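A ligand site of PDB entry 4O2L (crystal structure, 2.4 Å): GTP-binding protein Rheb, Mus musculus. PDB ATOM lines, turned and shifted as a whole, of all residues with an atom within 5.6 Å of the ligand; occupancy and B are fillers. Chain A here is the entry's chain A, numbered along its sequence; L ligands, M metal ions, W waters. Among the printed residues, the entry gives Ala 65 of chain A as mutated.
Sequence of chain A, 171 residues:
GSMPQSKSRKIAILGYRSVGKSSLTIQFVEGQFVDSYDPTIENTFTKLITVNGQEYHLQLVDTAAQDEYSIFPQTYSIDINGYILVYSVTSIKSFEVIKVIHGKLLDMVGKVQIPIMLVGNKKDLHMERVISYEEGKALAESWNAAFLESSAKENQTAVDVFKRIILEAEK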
ATOM      1  N   GLY A  15     -16.586  29.435 -22.581  1.00  0.00           N
ATOM      2  CA  GLY A  15     -17.835  29.630 -21.850  1.00  0.00           C
ATOM      3  C   GLY A  15     -18.025  31.028 -21.285  1.00  0.00           C
ATOM      4  O   GLY A  15     -17.132  31.878 -21.346  1.00  0.00           O
ATOM      5  N   TYR A  16     -19.199  31.236 -20.715  1.00  0.00           N
ATOM      6  CA  TYR A  16     -19.630  32.516 -20.151  1.00  0.00           C
ATOM      7  C   TYR A  16     -18.876  32.828 -18.861  1.00  0.00           C
ATOM      8  O   TYR A  16     -18.222  31.942 -18.286  1.00  0.00           O
ATOM      9  CB  TYR A  16     -21.145  32.440 -19.898  1.00  0.00           C
ATOM     10  CG  TYR A  16     -21.816  33.697 -19.402  1.00  0.00           C
ATOM     11  CD1 TYR A  16     -22.017  34.784 -20.247  1.00  0.00           C
ATOM     12  CD2 TYR A  16     -22.304  33.763 -18.103  1.00  0.00           C
ATOM     13  CE1 TYR A  16     -22.649  35.937 -19.792  1.00  0.00           C
ATOM     14  CE2 TYR A  16     -22.950  34.915 -17.646  1.00  0.00           C
ATOM     15  CZ  TYR A  16     -23.115  35.993 -18.492  1.00  0.00           C
ATOM     16  OH  TYR A  16     -23.766  37.122 -18.041  1.00  0.00           O
ATOM     17  N   ARG A  17     -18.966  34.080 -18.409  1.00  0.00           N
ATOM     18  CA  ARG A  17     -18.239  34.496 -17.212  1.00  0.00           C
ATOM     19  C   ARG A  17     -18.655  33.719 -15.971  1.00  0.00           C
ATOM     20  O   ARG A  17     -19.844  33.395 -15.800  1.00  0.00           O
ATOM     21  CB  ARG A  17     -18.360  35.995 -16.970  1.00  0.00           C
ATOM     22  CG  ARG A  17     -19.774  36.547 -17.067  1.00  0.00           C
ATOM     23  CD  ARG A  17     -19.808  38.047 -16.749  1.00  0.00           C
ATOM     24  NE  ARG A  17     -20.813  38.761 -17.534  1.00  0.00           N
ATOM     25  CZ  ARG A  17     -20.666  39.104 -18.825  1.00  0.00           C
ATOM     26  NH1 ARG A  17     -19.557  38.783 -19.491  1.00  0.00           N
ATOM     27  NH2 ARG A  17     -21.642  39.755 -19.457  1.00  0.00           N
ATOM     28  N   SER A  18     -17.664  33.418 -15.129  1.00  0.00           N
ATOM     29  CA  SER A  18     -17.870  32.773 -13.828  1.00  0.00           C
ATOM     30  C   SER A  18     -18.498  31.386 -13.854  1.00  0.00           C
ATOM     31  O   SER A  18     -19.027  30.951 -12.846  1.00  0.00           O
ATOM     32  CB  SER A  18     -18.692  33.676 -12.903  1.00  0.00           C
ATOM     33  OG  SER A  18     -17.952  34.821 -12.508  1.00  0.00           O
ATOM     34  N   VAL A  19     -18.443  30.675 -14.980  1.00  0.00           N
ATOM     35  CA  VAL A  19     -19.021  29.339 -15.025  1.00  0.00           C
ATOM     36  C   VAL A  19     -18.091  28.306 -14.386  1.00  0.00           C
ATOM     37  O   VAL A  19     -18.500  27.183 -14.101  1.00  0.00           O
ATOM     38  CB  VAL A  19     -19.382  28.895 -16.469  1.00  0.00           C
ATOM     39  CG1 VAL A  19     -20.447  29.810 -17.064  1.00  0.00           C
ATOM     40  CG2 VAL A  19     -18.123  28.801 -17.355  1.00  0.00           C
ATOM     41  N   GLY A  20     -16.843  28.713 -14.158  1.00  0.00           N
ATOM     42  CA  GLY A  20     -15.828  27.854 -13.586  1.00  0.00           C
ATOM     43  C   GLY A  20     -14.760  27.357 -14.560  1.00  0.00           C
ATOM     44  O   GLY A  20     -14.129  26.326 -14.298  1.00  0.00           O
ATOM     45  N   LYS A  21     -14.537  28.062 -15.669  1.00  0.00           N
ATOM     46  CA  LYS A  21     -13.502  27.643 -16.626  1.00  0.00           C
ATOM     47  C   LYS A  21     -12.140  27.529 -15.959  1.00  0.00           C
ATOM     48  O   LYS A  21     -11.427  26.546 -16.143  1.00  0.00           O
ATOM     49  CB  LYS A  21     -13.396  28.624 -17.800  1.00  0.00           C
ATOM     50  CG  LYS A  21     -14.658  28.738 -18.656  1.00  0.00           C
ATOM     51  CD  LYS A  21     -14.384  29.536 -19.933  1.00  0.00           C
ATOM     52  CE  LYS A  21     -14.013  30.979 -19.617  1.00  0.00           C
ATOM     53  NZ  LYS A  21     -15.113  31.675 -18.904  1.00  0.00           N
ATOM     54  N   SER A  22     -11.774  28.545 -15.183  1.00  0.00           N
ATOM     55  CA  SER A  22     -10.482  28.561 -14.539  1.00  0.00           C
ATOM     56  C   SER A  22     -10.404  27.539 -13.406  1.00  0.00           C
ATOM     57  O   SER A  22      -9.438  26.774 -13.325  1.00  0.00           O
ATOM     58  CB  SER A  22     -10.142  29.950 -14.025  1.00  0.00           C
ATOM     59  OG  SER A  22     -10.067  30.856 -15.098  1.00  0.00           O
ATOM     60  N   SER A  23     -11.405  27.537 -12.530  1.00  0.00           N
ATOM     61  CA  SER A  23     -11.429  26.619 -11.398  1.00  0.00           C
ATOM     62  C   SER A  23     -11.257  25.143 -11.802  1.00  0.00           C
ATOM     63  O   SER A  23     -10.470  24.415 -11.197  1.00  0.00           O
ATOM     64  CB  SER A  23     -12.696  26.806 -10.591  1.00  0.00           C
ATOM     65  OG  SER A  23     -12.700  28.075  -9.984  1.00  0.00           O
ATOM     66  N   LEU A  24     -11.988  24.730 -12.837  1.00  0.00           N
ATOM     67  CA  LEU A  24     -11.902  23.373 -13.350  1.00  0.00           C
ATOM     68  C   LEU A  24     -10.487  23.070 -13.819  1.00  0.00           C
ATOM     69  O   LEU A  24      -9.898  22.031 -13.491  1.00  0.00           O
ATOM     70  CB  LEU A  24     -12.861  23.181 -14.528  1.00  0.00           C
ATOM     71  CG  LEU A  24     -14.237  22.564 -14.277  1.00  0.00           C
ATOM     72  CD1 LEU A  24     -14.921  22.387 -15.598  1.00  0.00           C
ATOM     73  CD2 LEU A  24     -14.135  21.228 -13.541  1.00  0.00           C
ATOM     74  N   PHE A  33      -8.758  23.928  -5.352  1.00  0.00           N
ATOM     75  CA  PHE A  33      -9.904  24.777  -5.633  1.00  0.00           C
ATOM     76  C   PHE A  33      -9.679  26.192  -5.103  1.00  0.00           C
ATOM     77  O   PHE A  33      -9.234  26.400  -3.975  1.00  0.00           O
ATOM     78  CB  PHE A  33     -11.194  24.157  -5.059  1.00  0.00           C
ATOM     79  CG  PHE A  33     -12.418  25.016  -5.264  1.00  0.00           C
ATOM     80  CD1 PHE A  33     -12.965  25.170  -6.519  1.00  0.00           C
ATOM     81  CD2 PHE A  33     -13.003  25.659  -4.204  1.00  0.00           C
ATOM     82  CE1 PHE A  33     -14.080  25.955  -6.701  1.00  0.00           C
ATOM     83  CE2 PHE A  33     -14.125  26.437  -4.390  1.00  0.00           C
ATOM     84  CZ  PHE A  33     -14.656  26.586  -5.639  1.00  0.00           C
ATOM     85  N   VAL A  34      -9.997  27.159  -5.935  1.00  0.00           N
ATOM     86  CA  VAL A  34      -9.725  28.555  -5.706  1.00  0.00           C
ATOM     87  C   VAL A  34     -11.032  29.349  -5.753  1.00  0.00           C
ATOM     88  O   VAL A  34     -11.941  29.029  -6.522  1.00  0.00           O
ATOM     89  CB  VAL A  34      -8.796  29.050  -6.790  1.00  0.00           C
ATOM     90  CG1 VAL A  34      -7.352  28.681  -6.481  1.00  0.00           C
ATOM     91  CG2 VAL A  34      -9.210  28.379  -8.059  1.00  0.00           C
ATOM     92  N   ASP A  35     -11.115  30.397  -4.934  1.00  0.00           N
ATOM     93  CA  ASP A  35     -12.352  31.171  -4.813  1.00  0.00           C
ATOM     94  C   ASP A  35     -12.408  32.430  -5.700  1.00  0.00           C
ATOM     95  O   ASP A  35     -13.468  33.030  -5.849  1.00  0.00           O
ATOM     96  CB  ASP A  35     -12.587  31.527  -3.334  1.00  0.00           C
ATOM     97  CG  ASP A  35     -12.616  30.289  -2.426  1.00  0.00           C
ATOM     98  OD1 ASP A  35     -11.561  29.632  -2.232  1.00  0.00           O
ATOM     99  OD2 ASP A  35     -13.703  29.979  -1.908  1.00  0.00           O
ATOM    100  N   SER A  36     -11.281  32.814  -6.309  1.00  0.00           N
ATOM    101  CA  SER A  36     -11.195  34.069  -7.081  1.00  0.00           C
ATOM    102  C   SER A  36     -10.124  34.009  -8.206  1.00  0.00           C
ATOM    103  O   SER A  36      -9.297  33.095  -8.209  1.00  0.00           O
ATOM    104  CB  SER A  36     -10.941  35.256  -6.156  1.00  0.00           C
ATOM    105  OG  SER A  36     -10.811  36.485  -6.865  1.00  0.00           O
ATOM    106  N   TYR A  37     -10.135  35.008  -9.080  1.00  0.00           N
ATOM    107  CA  TYR A  37      -9.473  34.909 -10.386  1.00  0.00           C
ATOM    108  C   TYR A  37      -9.384  36.243 -11.132  1.00  0.00           C
ATOM    109  O   TYR A  37      -9.837  37.278 -10.637  1.00  0.00           O
ATOM    110  CB  TYR A  37     -10.259  33.927 -11.254  1.00  0.00           C
ATOM    111  CG  TYR A  37     -11.699  34.354 -11.477  1.00  0.00           C
ATOM    112  CD1 TYR A  37     -12.119  34.801 -12.722  1.00  0.00           C
ATOM    113  CD2 TYR A  37     -12.650  34.314 -10.444  1.00  0.00           C
ATOM    114  CE1 TYR A  37     -13.432  35.190 -12.934  1.00  0.00           C
ATOM    115  CE2 TYR A  37     -13.957  34.698 -10.661  1.00  0.00           C
ATOM    116  CZ  TYR A  37     -14.342  35.143 -11.915  1.00  0.00           C
ATOM    117  OH  TYR A  37     -15.644  35.535 -12.152  1.00  0.00           O
ATOM    118  N   ASP A  38      -8.795  36.210 -12.330  1.00  0.00           N
ATOM    119  CA  ASP A  38      -8.671  37.383 -13.203  1.00  0.00           C
ATOM    120  C   ASP A  38      -9.489  37.110 -14.461  1.00  0.00           C
ATOM    121  O   ASP A  38      -8.952  36.675 -15.472  1.00  0.00           O
ATOM    122  CB  ASP A  38      -7.212  37.616 -13.578  1.00  0.00           C
ATOM    123  CG  ASP A  38      -6.262  37.385 -12.421  1.00  0.00           C
ATOM    124  OD1 ASP A  38      -5.920  38.383 -11.734  1.00  0.00           O
ATOM    125  OD2 ASP A  38      -5.866  36.216 -12.190  1.00  0.00           O
ATOM    126  N   PRO A  39     -10.798  37.390 -14.397  1.00  0.00           N
ATOM    127  CA  PRO A  39     -11.867  37.038 -15.347  1.00  0.00           C
ATOM    128  C   PRO A  39     -11.596  37.233 -16.849  1.00  0.00           C
ATOM    129  O   PRO A  39     -11.893  36.317 -17.647  1.00  0.00           O
ATOM    130  CB  PRO A  39     -13.041  37.929 -14.892  1.00  0.00           C
ATOM    131  CG  PRO A  39     -12.486  38.887 -13.870  1.00  0.00           C
ATOM    132  CD  PRO A  39     -11.310  38.189 -13.273  1.00  0.00           C
ATOM    133  N   THR A  40     -11.075  38.397 -17.251  1.00  0.00           N
ATOM    134  CA  THR A  40     -10.922  38.762 -18.669  1.00  0.00           C
ATOM    135  C   THR A  40      -9.490  38.545 -19.175  1.00  0.00           C
ATOM    136  O   THR A  40      -9.046  39.186 -20.142  1.00  0.00           O
ATOM    137  CB  THR A  40     -11.355  40.238 -18.927  1.00  0.00           C
ATOM    138  OG1 THR A  40     -10.450  41.141 -18.264  1.00  0.00           O
ATOM    139  CG2 THR A  40     -12.776  40.490 -18.419  1.00  0.00           C
ATOM    140  N   ASP A  62      -7.119  28.372 -21.163  1.00  0.00           N
ATOM    141  CA  ASP A  62      -8.215  28.843 -20.335  1.00  0.00           C
ATOM    142  C   ASP A  62      -8.615  30.234 -20.813  1.00  0.00           C
ATOM    143  O   ASP A  62      -8.045  31.242 -20.383  1.00  0.00           O
ATOM    144  CB  ASP A  62      -7.788  28.866 -18.871  1.00  0.00           C
ATOM    145  CG  ASP A  62      -8.825  29.509 -17.952  1.00  0.00           C
ATOM    146  OD1 ASP A  62     -10.031  29.394 -18.221  1.00  0.00           O
ATOM    147  OD2 ASP A  62      -8.420  30.120 -16.941  1.00  0.00           O
ATOM    148  N   THR A  63      -9.591  30.286 -21.708  1.00  0.00           N
ATOM    149  CA  THR A  63      -9.903  31.506 -22.423  1.00  0.00           C
ATOM    150  C   THR A  63     -10.624  32.501 -21.544  1.00  0.00           C
ATOM    151  O   THR A  63     -11.168  32.142 -20.496  1.00  0.00           O
ATOM    152  CB  THR A  63     -10.714  31.228 -23.687  1.00  0.00           C
ATOM    153  OG1 THR A  63     -12.030  30.825 -23.309  1.00  0.00           O
ATOM    154  CG2 THR A  63     -10.065  30.136 -24.515  1.00  0.00           C
ATOM    155  N   ALA A  64     -10.597  33.761 -21.947  1.00  0.00           N
ATOM    156  CA  ALA A  64     -11.294  34.826 -21.251  1.00  0.00           C
ATOM    157  C   ALA A  64     -12.784  34.657 -21.486  1.00  0.00           C
ATOM    158  O   ALA A  64     -13.205  34.025 -22.459  1.00  0.00           O
ATOM    159  CB  ALA A  64     -10.827  36.173 -21.740  1.00  0.00           C
ATOM    160  N   ALA A  65     -13.593  35.208 -20.580  1.00  0.00           N
ATOM    161  CA  ALA A  65     -15.034  35.061 -20.676  1.00  0.00           C
ATOM    162  C   ALA A  65     -15.569  35.543 -22.028  1.00  0.00           C
ATOM    163  O   ALA A  65     -15.142  36.580 -22.531  1.00  0.00           O
ATOM    164  CB  ALA A  65     -15.724  35.804 -19.526  1.00  0.00           C
ATOM    165  N   ASN A 121     -20.907  22.661 -15.158  1.00  0.00           N
ATOM    166  CA  ASN A 121     -20.119  22.732 -13.943  1.00  0.00           C
ATOM    167  C   ASN A 121     -20.930  23.222 -12.720  1.00  0.00           C
ATOM    168  O   ASN A 121     -22.049  23.738 -12.887  1.00  0.00           O
ATOM    169  CB  ASN A 121     -18.909  23.650 -14.177  1.00  0.00           C
ATOM    170  CG  ASN A 121     -17.900  23.588 -13.060  1.00  0.00           C
ATOM    171  OD1 ASN A 121     -17.595  22.507 -12.556  1.00  0.00           O
ATOM    172  ND2 ASN A 121     -17.397  24.755 -12.656  1.00  0.00           N
ATOM    173  N   LYS A 122     -20.354  23.058 -11.530  1.00  0.00           N
ATOM    174  CA  LYS A 122     -20.952  23.478 -10.246  1.00  0.00           C
ATOM    175  C   LYS A 122     -22.081  22.565  -9.853  1.00  0.00           C
ATOM    176  O   LYS A 122     -23.025  23.001  -9.227  1.00  0.00           O
ATOM    177  CB  LYS A 122     -21.448  24.940 -10.254  1.00  0.00           C
ATOM    178  CG  LYS A 122     -20.448  25.957 -10.761  1.00  0.00           C
ATOM    179  CD  LYS A 122     -20.838  27.392 -10.417  1.00  0.00           C
ATOM    180  CE  LYS A 122     -19.797  28.358 -10.973  1.00  0.00           C
ATOM    181  NZ  LYS A 122     -20.138  29.776 -10.718  1.00  0.00           N
ATOM    182  N   LYS A 123     -21.953  21.284 -10.192  1.00  0.00           N
ATOM    183  CA  LYS A 123     -22.981  20.312  -9.839  1.00  0.00           C
ATOM    184  C   LYS A 123     -23.127  20.149  -8.334  1.00  0.00           C
ATOM    185  O   LYS A 123     -24.160  19.655  -7.860  1.00  0.00           O
ATOM    186  CB  LYS A 123     -22.742  18.967 -10.501  1.00  0.00           C
ATOM    187  CG  LYS A 123     -21.582  18.160  -9.939  1.00  0.00           C
ATOM    188  CD  LYS A 123     -21.508  16.830 -10.662  1.00  0.00           C
ATOM    189  CE  LYS A 123     -20.330  16.021 -10.184  1.00  0.00           C
ATOM    190  NZ  LYS A 123     -20.426  15.704  -8.737  1.00  0.00           N
ATOM    191  N   ASP A 124     -22.108  20.572  -7.591  1.00  0.00           N
ATOM    192  CA  ASP A 124     -22.110  20.506  -6.137  1.00  0.00           C
ATOM    193  C   ASP A 124     -23.056  21.513  -5.469  1.00  0.00           C
ATOM    194  O   ASP A 124     -23.360  21.392  -4.267  1.00  0.00           O
ATOM    195  CB  ASP A 124     -20.696  20.719  -5.588  1.00  0.00           C
ATOM    196  CG  ASP A 124     -20.144  22.096  -5.937  1.00  0.00           C
ATOM    197  OD1 ASP A 124     -19.628  22.256  -7.066  1.00  0.00           O
ATOM    198  OD2 ASP A 124     -20.210  23.003  -5.080  1.00  0.00           O
ATOM    199  N   LEU A 125     -23.483  22.524  -6.219  1.00  0.00           N
ATOM    200  CA  LEU A 125     -24.377  23.538  -5.661  1.00  0.00           C
ATOM    201  C   LEU A 125     -25.824  23.127  -5.882  1.00  0.00           C
ATOM    202  O   LEU A 125     -26.536  23.737  -6.676  1.00  0.00           O
ATOM    203  CB  LEU A 125     -24.115  24.895  -6.315  1.00  0.00           C
ATOM    204  CG  LEU A 125     -22.741  25.497  -6.026  1.00  0.00           C
ATOM    205  CD1 LEU A 125     -22.556  26.858  -6.728  1.00  0.00           C
ATOM    206  CD2 LEU A 125     -22.511  25.613  -4.528  1.00  0.00           C
ATOM    207  N   SER A 150     -19.770  18.487 -13.711  1.00  0.00           N
ATOM    208  CA  SER A 150     -18.514  18.578 -13.013  1.00  0.00           C
ATOM    209  C   SER A 150     -18.649  19.486 -11.814  1.00  0.00           C
ATOM    210  O   SER A 150     -19.598  20.251 -11.741  1.00  0.00           O
ATOM    211  CB  SER A 150     -17.436  19.118 -13.942  1.00  0.00           C
ATOM    212  OG  SER A 150     -17.669  20.488 -14.219  1.00  0.00           O
ATOM    213  N   SER A 151     -17.706  19.354 -10.888  1.00  0.00           N
ATOM    214  CA  SER A 151     -17.507  20.309  -9.804  1.00  0.00           C
ATOM    215  C   SER A 151     -16.018  20.559  -9.645  1.00  0.00           C
ATOM    216  O   SER A 151     -15.246  19.620  -9.450  1.00  0.00           O
ATOM    217  CB  SER A 151     -18.055  19.765  -8.476  1.00  0.00           C
ATOM    218  OG  SER A 151     -17.727  20.619  -7.394  1.00  0.00           O
ATOM    219  N   ALA A 152     -15.614  21.828  -9.729  1.00  0.00           N
ATOM    220  CA  ALA A 152     -14.211  22.198  -9.547  1.00  0.00           C
ATOM    221  C   ALA A 152     -13.698  21.900  -8.129  1.00  0.00           C
ATOM    222  O   ALA A 152     -12.496  21.953  -7.884  1.00  0.00           O
ATOM    223  CB  ALA A 152     -13.999  23.636  -9.888  1.00  0.00           C
ATOM    224  N   LYS A 153     -14.602  21.577  -7.208  1.00  0.00           N
ATOM    225  CA  LYS A 153     -14.222  21.148  -5.862  1.00  0.00           C
ATOM    226  C   LYS A 153     -13.855  19.672  -5.803  1.00  0.00           C
ATOM    227  O   LYS A 153     -13.270  19.201  -4.830  1.00  0.00           O
ATOM    228  CB  LYS A 153     -15.361  21.406  -4.876  1.00  0.00           C
ATOM    229  CG  LYS A 153     -15.630  22.866  -4.586  1.00  0.00           C
ATOM    230  CD  LYS A 153     -16.782  22.996  -3.612  1.00  0.00           C
ATOM    231  CE  LYS A 153     -16.933  24.389  -3.085  1.00  0.00           C
ATOM    232  NZ  LYS A 153     -18.052  24.443  -2.074  1.00  0.00           N
HETATM  233  P1  LIG L   1     -14.085  34.020 -16.004  1.00  0.00           P
HETATM  234  O1  LIG L   1     -14.610  35.370 -15.588  1.00  0.00           O
HETATM  235  O2  LIG L   1     -14.369  33.805 -17.482  1.00  0.00           O
HETATM  236  O3  LIG L   1     -12.601  33.915 -15.771  1.00  0.00           O
HETATM  237  O4  LIG L   1     -14.910  32.951 -15.126  1.00  0.00           O
HETATM  238  P2  LIG L   1     -14.485  31.392 -14.989  1.00  0.00           P
HETATM  239  O5  LIG L   1     -12.988  31.188 -15.103  1.00  0.00           O
HETATM  240  O6  LIG L   1     -15.235  30.644 -16.063  1.00  0.00           O
HETATM  241  O7  LIG L   1     -15.035  30.981 -13.523  1.00  0.00           O
HETATM  242  P3  LIG L   1     -14.127  30.769 -12.212  1.00  0.00           P
HETATM  243  O8  LIG L   1     -13.293  31.983 -11.946  1.00  0.00           O
HETATM  244  O9  LIG L   1     -13.265  29.536 -12.329  1.00  0.00           O
HETATM  245  O10 LIG L   1     -15.215  30.666 -11.035  1.00  0.00           O
HETATM  246  C1  LIG L   1     -16.163  31.693 -10.824  1.00  0.00           C
HETATM  247  C2  LIG L   1     -16.594  31.548  -9.369  1.00  0.00           C
HETATM  248  O11 LIG L   1     -17.277  30.309  -9.263  1.00  0.00           O
HETATM  249  C3  LIG L   1     -15.397  31.463  -8.438  1.00  0.00           C
HETATM  250  O12 LIG L   1     -15.727  32.175  -7.275  1.00  0.00           O
HETATM  251  C4  LIG L   1     -15.257  29.989  -8.112  1.00  0.00           C
HETATM  252  O13 LIG L   1     -14.723  29.790  -6.813  1.00  0.00           O
HETATM  253  C5  LIG L   1     -16.682  29.472  -8.281  1.00  0.00           C
HETATM  254  N1  LIG L   1     -16.754  28.092  -8.810  1.00  0.00           N
HETATM  255  C6  LIG L   1     -16.229  27.665  -9.995  1.00  0.00           C
HETATM  256  N2  LIG L   1     -16.512  26.342 -10.136  1.00  0.00           N
HETATM  257  C7  LIG L   1     -17.219  25.911  -9.065  1.00  0.00           C
HETATM  258  C8  LIG L   1     -17.760  24.668  -8.712  1.00  0.00           C
HETATM  259  O14 LIG L   1     -17.624  23.687  -9.446  1.00  0.00           O
HETATM  260  N3  LIG L   1     -18.444  24.538  -7.528  1.00  0.00           N
HETATM  261  C9  LIG L   1     -18.599  25.625  -6.688  1.00  0.00           C
HETATM  262  N4  LIG L   1     -19.260  25.494  -5.548  1.00  0.00           N
HETATM  263  N5  LIG L   1     -18.065  26.862  -7.045  1.00  0.00           N
HETATM  264  C10 LIG L   1     -17.388  27.008  -8.215  1.00  0.00           C
HETATM  265 MG    MG M   1     -11.455  31.874 -17.398  1.00  0.00          MG
HETATM  266  O   HOH W   1     -14.863  35.224  -7.973  1.00  0.00           O
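Water W1 lies within hydrogen-bond range of O12 of the ligand (3.2 Å) and O of Asp 35 (3.4 Å).
N of Lys 21 sits at hydrogen-bond distance from O6 of the ligand (2.7 Å).
The backbone NH (N) of Ser 22 is in hydrogen-bond range of an oxygen (O5) of the ligand, 2.9 Å away.
O12 of the ligand lies within hydrogen-bond range of O of Asp 35.
OG of Ser 22 lies within hydrogen-bond range of O5 of the ligand, 2.9 Å away.
The backbone NH (N) of Lys 122 sits close to an oxygen (O14) of the ligand (3.5 Å).
NZ of Lys 21 is in salt-bridge range of O2 of the ligand, 2.7 Å away.
The backbone NH (N) of Ala 65 sits close to an oxygen (O2) of the ligand, at 3.5 Å.
An oxygen (O11) of the ligand lies within hydrogen-bond range of the side-chain amino group of Lys 122 (3.3 Å).
The side-chain amide nitrogen (ND2) of Asn 121 is in hydrogen-bond range of a nitrogen (N2) of the ligand, at 3.1 Å.
O14 of the ligand sits at hydrogen-bond distance from N of Ala 152, 2.8 Å away.
An oxygen (O9) of the ligand is in hydrogen-bond range of the side-chain hydroxyl (OG) of Ser 23, at 2.8 Å.
N of Val 19 sits at hydrogen-bond distance from O6 of the ligand (3.4 Å).
The backbone carbonyl oxygen (O) of Val 34 is in hydrogen-bond range of an oxygen (O13) of the ligand.
O9 of the ligand lies within hydrogen-bond range of N of Ser 23 (2.7 Å).
N of Ser 18 sits at hydrogen-bond distance from O4 of the ligand (2.8 Å).
OD1 of Asp 124 is in hydrogen-bond range of N3 of the ligand.
The backbone NH (N) of Gly 20 lies within hydrogen-bond range of an oxygen (O7) of the ligand.
O of Ser 18 lies within hydrogen-bond range of NZ of Lys 122 (2.7 Å).
O of Tyr 16 is in hydrogen-bond range of NZ of Lys 21 (3.2 Å).
The side-chain hydroxyl of Ser 22 sits at hydrogen-bond distance from the side-chain carboxylate of Asp 62 (2.6 Å).
The side-chain amino group of Lys 21 lies within hydrogen-bond range of the backbone carbonyl oxygen of Gly 15, at 3.2 Å.
OD2 of Asp 124 is in salt-bridge range of NZ of Lys 153.
The side-chain amide oxygen (OD1) of Asn 121 sits at hydrogen-bond distance from the side-chain hydroxyl (OG) of Ser 150, at 2.6 Å.
The backbone NH (N) of Lys 122 lies within hydrogen-bond range of the backbone carbonyl oxygen (O) of Ser 150 (2.9 Å).
The side-chain amide nitrogen of Asn 121 lies within hydrogen-bond range of the backbone carbonyl oxygen of Val 19 (3.0 Å).
The backbone carbonyl oxygen (O) of Pro 39 lies close to an oxygen (O3) of the ligand (3.1 Å).
Tyr 16 touches the ligand (O to O6, 3.9 Å).
C of Arg 17 touches O4 of the ligand, at 3.9 Å.
Phe 33 touches the ligand.
CD2 of Tyr 37 touches O8 of the ligand, 2.8 Å away.
Leu 125 touches the ligand.
CA of Ser 151 touches O14 of the ligand (3.4 Å).
Lys 153 touches the ligand (CE to N4, 3.6 Å).
Hydrophobic or aromatic side chains that line the ligand: Val 19, Phe 33, Tyr 37, Pro 39, Ala 65, Leu 125 and Ala 152.
Of the 31 residues printed, 21 come within 4 Å of the ligand.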
